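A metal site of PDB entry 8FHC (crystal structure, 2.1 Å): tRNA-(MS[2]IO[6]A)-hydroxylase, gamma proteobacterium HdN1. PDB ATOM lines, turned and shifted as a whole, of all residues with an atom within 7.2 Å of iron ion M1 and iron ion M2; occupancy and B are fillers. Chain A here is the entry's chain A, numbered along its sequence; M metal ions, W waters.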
ATOM      1  N   HIS A  42      29.000   1.792 -15.636  1.00  0.00           N
ATOM      2  CA  HIS A  42      28.567   2.233 -16.948  1.00  0.00           C
ATOM      3  C   HIS A  42      28.694   3.753 -17.029  1.00  0.00           C
ATOM      4  O   HIS A  42      29.400   4.266 -17.889  1.00  0.00           O
ATOM      5  CB  HIS A  42      27.162   1.682 -17.258  1.00  0.00           C
ATOM      6  CG  HIS A  42      26.598   2.116 -18.559  1.00  0.00           C
ATOM      7  ND1 HIS A  42      25.326   1.737 -18.908  1.00  0.00           N
ATOM      8  CD2 HIS A  42      27.046   2.876 -19.566  1.00  0.00           C
ATOM      9  CE1 HIS A  42      25.021   2.273 -20.084  1.00  0.00           C
ATOM     10  NE2 HIS A  42      26.036   2.987 -20.498  1.00  0.00           N
ATOM     11  N   CYS A  45      32.217   4.707 -17.475  1.00  0.00           N
ATOM     12  CA  CYS A  45      32.743   4.375 -18.777  1.00  0.00           C
ATOM     13  C   CYS A  45      32.377   5.414 -19.824  1.00  0.00           C
ATOM     14  O   CYS A  45      33.159   5.648 -20.719  1.00  0.00           O
ATOM     15  CB  CYS A  45      32.217   3.026 -19.267  1.00  0.00           C
ATOM     16  SG  CYS A  45      33.021   1.678 -18.387  1.00  0.00           S
ATOM     17  N   GLU A  46      31.151   5.944 -19.751  1.00  0.00           N
ATOM     18  CA  GLU A  46      30.698   6.955 -20.675  1.00  0.00           C
ATOM     19  C   GLU A  46      31.545   8.228 -20.529  1.00  0.00           C
ATOM     20  O   GLU A  46      31.914   8.836 -21.525  1.00  0.00           O
ATOM     21  CB  GLU A  46      29.236   7.290 -20.438  1.00  0.00           C
ATOM     22  CG  GLU A  46      28.294   6.121 -20.573  1.00  0.00           C
ATOM     23  CD  GLU A  46      28.056   5.618 -21.992  1.00  0.00           C
ATOM     24  OE1 GLU A  46      27.226   4.713 -22.164  1.00  0.00           O
ATOM     25  OE2 GLU A  46      28.623   6.204 -22.921  1.00  0.00           O
ATOM     26  N   ALA A  49      34.920   7.540 -22.121  1.00  0.00           N
ATOM     27  CA  ALA A  49      34.907   7.590 -23.566  1.00  0.00           C
ATOM     28  C   ALA A  49      34.921   9.061 -24.011  1.00  0.00           C
ATOM     29  O   ALA A  49      35.621   9.439 -24.945  1.00  0.00           O
ATOM     30  CB  ALA A  49      33.733   6.800 -24.079  1.00  0.00           C
ATOM     31  N   LEU A  73      31.363  12.488 -31.238  1.00  0.00           N
ATOM     32  CA  LEU A  73      31.368  11.330 -30.369  1.00  0.00           C
ATOM     33  C   LEU A  73      31.386  11.737 -28.887  1.00  0.00           C
ATOM     34  O   LEU A  73      30.615  11.199 -28.095  1.00  0.00           O
ATOM     35  CB  LEU A  73      32.565  10.472 -30.758  1.00  0.00           C
ATOM     36  CG  LEU A  73      32.494   9.007 -30.309  1.00  0.00           C
ATOM     37  CD1 LEU A  73      33.020   8.093 -31.414  1.00  0.00           C
ATOM     38  CD2 LEU A  73      33.276   8.808 -29.013  1.00  0.00           C
ATOM     39  N   GLU A  76      28.095  12.855 -27.643  1.00  0.00           N
ATOM     40  CA  GLU A  76      27.158  11.752 -27.504  1.00  0.00           C
ATOM     41  C   GLU A  76      27.467  10.965 -26.233  1.00  0.00           C
ATOM     42  O   GLU A  76      26.560  10.546 -25.519  1.00  0.00           O
ATOM     43  CB  GLU A  76      27.180  10.831 -28.723  1.00  0.00           C
ATOM     44  CG  GLU A  76      26.811  11.539 -30.006  1.00  0.00           C
ATOM     45  CD  GLU A  76      26.810  10.720 -31.278  1.00  0.00           C
ATOM     46  OE1 GLU A  76      26.932   9.472 -31.207  1.00  0.00           O
ATOM     47  OE2 GLU A  76      26.659  11.335 -32.350  1.00  0.00           O
ATOM     48  N   GLU A  77      28.751  10.794 -25.915  1.00  0.00           N
ATOM     49  CA  GLU A  77      29.129  10.033 -24.731  1.00  0.00           C
ATOM     50  C   GLU A  77      28.692  10.768 -23.461  1.00  0.00           C
ATOM     51  O   GLU A  77      28.300  10.145 -22.477  1.00  0.00           O
ATOM     52  CB  GLU A  77      30.631   9.789 -24.664  1.00  0.00           C
ATOM     53  CG  GLU A  77      31.216   9.016 -25.826  1.00  0.00           C
ATOM     54  CD  GLU A  77      30.709   7.590 -25.992  1.00  0.00           C
ATOM     55  OE1 GLU A  77      31.181   6.910 -26.906  1.00  0.00           O
ATOM     56  OE2 GLU A  77      29.821   7.177 -25.246  1.00  0.00           O
ATOM     57  N   LEU A  78      28.770  12.120 -23.472  1.00  0.00           N
ATOM     58  CA  LEU A  78      28.376  12.929 -22.323  1.00  0.00           C
ATOM     59  C   LEU A  78      26.873  12.841 -22.142  1.00  0.00           C
ATOM     60  O   LEU A  78      26.378  12.906 -21.022  1.00  0.00           O
ATOM     61  CB  LEU A  78      28.825  14.375 -22.534  1.00  0.00           C
ATOM     62  CG  LEU A  78      30.319  14.631 -22.310  1.00  0.00           C
ATOM     63  CD1 LEU A  78      30.735  16.015 -22.775  1.00  0.00           C
ATOM     64  CD2 LEU A  78      30.683  14.410 -20.836  1.00  0.00           C
ATOM     65  N   LEU A  79      26.148  12.747 -23.248  1.00  0.00           N
ATOM     66  CA  LEU A  79      24.703  12.577 -23.253  1.00  0.00           C
ATOM     67  C   LEU A  79      24.386  11.194 -22.658  1.00  0.00           C
ATOM     68  O   LEU A  79      23.514  11.076 -21.805  1.00  0.00           O
ATOM     69  CB  LEU A  79      24.249  12.700 -24.709  1.00  0.00           C
ATOM     70  CG  LEU A  79      22.941  13.420 -25.022  1.00  0.00           C
ATOM     71  CD1 LEU A  79      22.904  14.822 -24.461  1.00  0.00           C
ATOM     72  CD2 LEU A  79      22.787  13.508 -26.539  1.00  0.00           C
ATOM     73  N   HIS A  80      25.101  10.147 -23.109  1.00  0.00           N
ATOM     74  CA  HIS A  80      24.966   8.839 -22.485  1.00  0.00           C
ATOM     75  C   HIS A  80      25.169   8.946 -20.972  1.00  0.00           C
ATOM     76  O   HIS A  80      24.416   8.351 -20.218  1.00  0.00           O
ATOM     77  CB  HIS A  80      25.919   7.823 -23.127  1.00  0.00           C
ATOM     78  CG  HIS A  80      25.585   7.544 -24.555  1.00  0.00           C
ATOM     79  ND1 HIS A  80      26.419   6.863 -25.417  1.00  0.00           N
ATOM     80  CD2 HIS A  80      24.459   7.814 -25.238  1.00  0.00           C
ATOM     81  CE1 HIS A  80      25.833   6.767 -26.587  1.00  0.00           C
ATOM     82  NE2 HIS A  80      24.617   7.320 -26.487  1.00  0.00           N
ATOM     83  N   PHE A  81      26.173   9.710 -20.546  1.00  0.00           N
ATOM     84  CA  PHE A  81      26.480   9.872 -19.124  1.00  0.00           C
ATOM     85  C   PHE A  81      25.265  10.427 -18.371  1.00  0.00           C
ATOM     86  O   PHE A  81      24.848   9.866 -17.365  1.00  0.00           O
ATOM     87  CB  PHE A  81      27.696  10.768 -18.889  1.00  0.00           C
ATOM     88  CG  PHE A  81      27.917  11.154 -17.448  1.00  0.00           C
ATOM     89  CD1 PHE A  81      28.251  10.204 -16.495  1.00  0.00           C
ATOM     90  CD2 PHE A  81      27.724  12.459 -17.015  1.00  0.00           C
ATOM     91  CE1 PHE A  81      28.423  10.552 -15.159  1.00  0.00           C
ATOM     92  CE2 PHE A  81      27.859  12.801 -15.676  1.00  0.00           C
ATOM     93  CZ  PHE A  81      28.235  11.853 -14.757  1.00  0.00           C
ATOM     94  N   ILE A 129      36.918  -1.143 -27.669  1.00  0.00           N
ATOM     95  CA  ILE A 129      36.101  -0.798 -26.515  1.00  0.00           C
ATOM     96  C   ILE A 129      34.650  -0.603 -26.962  1.00  0.00           C
ATOM     97  O   ILE A 129      33.735  -1.058 -26.287  1.00  0.00           O
ATOM     98  CB  ILE A 129      36.656   0.426 -25.789  1.00  0.00           C
ATOM     99  CG1 ILE A 129      38.012   0.123 -25.158  1.00  0.00           C
ATOM    100  CG2 ILE A 129      35.678   0.938 -24.747  1.00  0.00           C
ATOM    101  CD1 ILE A 129      38.643   1.320 -24.517  1.00  0.00           C
ATOM    102  N   GLU A 130      34.450   0.077 -28.091  1.00  0.00           N
ATOM    103  CA  GLU A 130      33.097   0.428 -28.517  1.00  0.00           C
ATOM    104  C   GLU A 130      32.410  -0.839 -29.042  1.00  0.00           C
ATOM    105  O   GLU A 130      31.234  -1.068 -28.753  1.00  0.00           O
ATOM    106  CB  GLU A 130      33.146   1.536 -29.573  1.00  0.00           C
ATOM    107  CG  GLU A 130      33.633   2.902 -29.081  1.00  0.00           C
ATOM    108  CD  GLU A 130      32.800   3.586 -28.004  1.00  0.00           C
ATOM    109  OE1 GLU A 130      32.142   4.589 -28.313  1.00  0.00           O
ATOM    110  OE2 GLU A 130      32.835   3.162 -26.840  1.00  0.00           O
ATOM    111  N   SER A 133      31.466  -2.980 -25.890  1.00  0.00           N
ATOM    112  CA  SER A 133      30.309  -2.417 -25.231  1.00  0.00           C
ATOM    113  C   SER A 133      29.035  -2.790 -25.997  1.00  0.00           C
ATOM    114  O   SER A 133      28.033  -3.155 -25.387  1.00  0.00           O
ATOM    115  CB  SER A 133      30.439  -0.907 -25.063  1.00  0.00           C
ATOM    116  OG  SER A 133      31.628  -0.587 -24.342  1.00  0.00           O
ATOM    117  N   PHE A 137      26.124  -4.861 -24.292  1.00  0.00           N
ATOM    118  CA  PHE A 137      24.767  -4.345 -24.198  1.00  0.00           C
ATOM    119  C   PHE A 137      23.808  -5.308 -24.887  1.00  0.00           C
ATOM    120  O   PHE A 137      22.690  -5.490 -24.421  1.00  0.00           O
ATOM    121  CB  PHE A 137      24.625  -2.944 -24.803  1.00  0.00           C
ATOM    122  CG  PHE A 137      25.351  -1.805 -24.127  1.00  0.00           C
ATOM    123  CD1 PHE A 137      25.308  -1.625 -22.750  1.00  0.00           C
ATOM    124  CD2 PHE A 137      26.034  -0.855 -24.874  1.00  0.00           C
ATOM    125  CE1 PHE A 137      25.959  -0.552 -22.147  1.00  0.00           C
ATOM    126  CE2 PHE A 137      26.694   0.200 -24.267  1.00  0.00           C
ATOM    127  CZ  PHE A 137      26.670   0.341 -22.904  1.00  0.00           C
ATOM    128  N   TYR A 156      16.845   0.741 -22.890  1.00  0.00           N
ATOM    129  CA  TYR A 156      17.939   1.687 -23.065  1.00  0.00           C
ATOM    130  C   TYR A 156      19.149   0.978 -23.679  1.00  0.00           C
ATOM    131  O   TYR A 156      19.807   1.547 -24.539  1.00  0.00           O
ATOM    132  CB  TYR A 156      18.284   2.338 -21.733  1.00  0.00           C
ATOM    133  CG  TYR A 156      19.373   3.377 -21.840  1.00  0.00           C
ATOM    134  CD1 TYR A 156      19.291   4.407 -22.752  1.00  0.00           C
ATOM    135  CD2 TYR A 156      20.475   3.339 -20.994  1.00  0.00           C
ATOM    136  CE1 TYR A 156      20.288   5.370 -22.841  1.00  0.00           C
ATOM    137  CE2 TYR A 156      21.481   4.284 -21.080  1.00  0.00           C
ATOM    138  CZ  TYR A 156      21.396   5.309 -22.004  1.00  0.00           C
ATOM    139  OH  TYR A 156      22.408   6.254 -22.053  1.00  0.00           O
ATOM    140  N   LEU A 160      21.081   1.848 -27.216  1.00  0.00           N
ATOM    141  CA  LEU A 160      22.493   2.218 -27.312  1.00  0.00           C
ATOM    142  C   LEU A 160      23.225   1.493 -28.441  1.00  0.00           C
ATOM    143  O   LEU A 160      24.317   1.933 -28.823  1.00  0.00           O
ATOM    144  CB  LEU A 160      23.195   1.929 -25.981  1.00  0.00           C
ATOM    145  CG  LEU A 160      23.505   3.118 -25.067  1.00  0.00           C
ATOM    146  CD1 LEU A 160      22.618   4.312 -25.342  1.00  0.00           C
ATOM    147  CD2 LEU A 160      23.404   2.705 -23.613  1.00  0.00           C
ATOM    148  N   SER A 163      24.204   3.402 -31.582  1.00  0.00           N
ATOM    149  CA  SER A 163      25.219   4.373 -31.179  1.00  0.00           C
ATOM    150  C   SER A 163      26.608   3.752 -31.158  1.00  0.00           C
ATOM    151  O   SER A 163      27.531   4.243 -31.794  1.00  0.00           O
ATOM    152  CB  SER A 163      24.852   4.905 -29.800  1.00  0.00           C
ATOM    153  OG  SER A 163      25.486   6.139 -29.551  1.00  0.00           O
ATOM    154  N   GLU A 164      26.726   2.657 -30.409  1.00  0.00           N
ATOM    155  CA  GLU A 164      28.013   2.026 -30.161  1.00  0.00           C
ATOM    156  C   GLU A 164      28.570   1.449 -31.454  1.00  0.00           C
ATOM    157  O   GLU A 164      29.784   1.447 -31.641  1.00  0.00           O
ATOM    158  CB  GLU A 164      27.887   0.909 -29.122  1.00  0.00           C
ATOM    159  CG  GLU A 164      27.610   1.432 -27.731  1.00  0.00           C
ATOM    160  CD  GLU A 164      28.728   2.286 -27.165  1.00  0.00           C
ATOM    161  OE1 GLU A 164      29.740   2.464 -27.866  1.00  0.00           O
ATOM    162  OE2 GLU A 164      28.580   2.771 -26.024  1.00  0.00           O
ATOM    163  N   SER A 165      27.669   0.902 -32.304  1.00  0.00           N
ATOM    164  CA  SER A 165      28.050   0.322 -33.577  1.00  0.00           C
ATOM    165  C   SER A 165      28.697   1.382 -34.461  1.00  0.00           C
ATOM    166  O   SER A 165      29.754   1.145 -35.073  1.00  0.00           O
ATOM    167  CB  SER A 165      26.851  -0.285 -34.233  1.00  0.00           C
ATOM    168  OG  SER A 165      27.181  -0.757 -35.516  1.00  0.00           O
ATOM    169  N   HIS A 167      30.067   4.243 -33.325  1.00  0.00           N
ATOM    170  CA  HIS A 167      31.309   4.673 -32.686  1.00  0.00           C
ATOM    171  C   HIS A 167      32.456   3.737 -33.058  1.00  0.00           C
ATOM    172  O   HIS A 167      33.563   4.182 -33.353  1.00  0.00           O
ATOM    173  CB  HIS A 167      31.130   4.784 -31.166  1.00  0.00           C
ATOM    174  CG  HIS A 167      30.209   5.874 -30.719  1.00  0.00           C
ATOM    175  ND1 HIS A 167      29.811   6.020 -29.413  1.00  0.00           N
ATOM    176  CD2 HIS A 167      29.583   6.858 -31.383  1.00  0.00           C
ATOM    177  CE1 HIS A 167      28.995   7.067 -29.284  1.00  0.00           C
ATOM    178  NE2 HIS A 167      28.859   7.594 -30.474  1.00  0.00           N
ATOM    179  N   PHE A 168      32.199   2.426 -33.026  1.00  0.00           N
ATOM    180  CA  PHE A 168      33.162   1.405 -33.415  1.00  0.00           C
ATOM    181  C   PHE A 168      33.641   1.671 -34.848  1.00  0.00           C
ATOM    182  O   PHE A 168      34.852   1.669 -35.126  1.00  0.00           O
ATOM    183  CB  PHE A 168      32.503   0.024 -33.299  1.00  0.00           C
ATOM    184  CG  PHE A 168      33.003  -1.000 -34.275  1.00  0.00           C
ATOM    185  CD1 PHE A 168      34.284  -1.528 -34.161  1.00  0.00           C
ATOM    186  CD2 PHE A 168      32.198  -1.420 -35.331  1.00  0.00           C
ATOM    187  CE1 PHE A 168      34.748  -2.456 -35.086  1.00  0.00           C
ATOM    188  CE2 PHE A 168      32.670  -2.343 -36.252  1.00  0.00           C
ATOM    189  CZ  PHE A 168      33.937  -2.854 -36.133  1.00  0.00           C
ATOM    190  N   TYR A 171      35.840   4.892 -35.109  1.00  0.00           N
ATOM    191  CA  TYR A 171      37.192   4.688 -34.589  1.00  0.00           C
ATOM    192  C   TYR A 171      38.004   3.872 -35.590  1.00  0.00           C
ATOM    193  O   TYR A 171      39.113   4.250 -35.931  1.00  0.00           O
ATOM    194  CB  TYR A 171      37.140   4.093 -33.182  1.00  0.00           C
ATOM    195  CG  TYR A 171      37.213   5.126 -32.080  1.00  0.00           C
ATOM    196  CD1 TYR A 171      38.378   5.854 -31.865  1.00  0.00           C
ATOM    197  CD2 TYR A 171      36.148   5.357 -31.226  1.00  0.00           C
ATOM    198  CE1 TYR A 171      38.490   6.756 -30.825  1.00  0.00           C
ATOM    199  CE2 TYR A 171      36.239   6.280 -30.196  1.00  0.00           C
ATOM    200  CZ  TYR A 171      37.409   6.995 -30.001  1.00  0.00           C
ATOM    201  OH  TYR A 171      37.522   7.941 -29.016  1.00  0.00           O
HETATM  202 FE    FE M   1      28.257   5.814 -25.010  1.00  0.00          FE
HETATM  203 FE    FE M   2      30.400   4.998 -27.442  1.00  0.00          FE
HETATM  204  O   HOH W   1      30.442   4.359 -25.043  1.00  0.00           O
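Water W1 bridges the side-chain carboxylate of Glu 164 (2.6 Å) and the side-chain carboxylate of Glu 130 (3.2 Å).
Within 4 Å of iron ion M2: Glu 77, Glu 130, Glu 164 and His 167. The nearest printed residue that does not touch iron ion M2 is His 80 (4.8 Å).
Iron ion M2 is bound by OE1 of Glu 130 (2.0 Å), OE1 of Glu 77 (2.1 Å), ND1 of His 167 (2.3 Å) and water W1 (2.5 Å). Slightly farther from iron ion M2 lies OE1 of Glu 164 (2.7 Å).
Iron ion M1 is bound by OE2 of Glu 77 (2.1 Å), ND1 of His 80 (2.2 Å) and OE2 of Glu 46 (2.2 Å). Slightly farther from iron ion M1 lies water W1 (2.6 Å).
Of the 23 residues printed, 4 come within 4 Å of iron ion M1. Along chain A the residues within 4 Å of iron ion M1 span positions 46 to 164. The nearest printed residue that does not touch iron ion M1 is His 167 (4.5 Å).
OG of Ser 163 lies close to NE2 of His 80 (3.4 Å). The side-chain carboxylate of Glu 46 lies within hydrogen-bond range of a ring nitrogen (NE2) of His 42 (2.7 Å). The backbone carbonyl oxygen of His 80 is in hydrogen-bond range of the side-chain hydroxyl of Tyr 156 (3.4 Å). The side-chain carboxylate (OE1) of Glu 76 is in hydrogen-bond range of a ring nitrogen (NE2) of His 167, 2.8 Å away.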
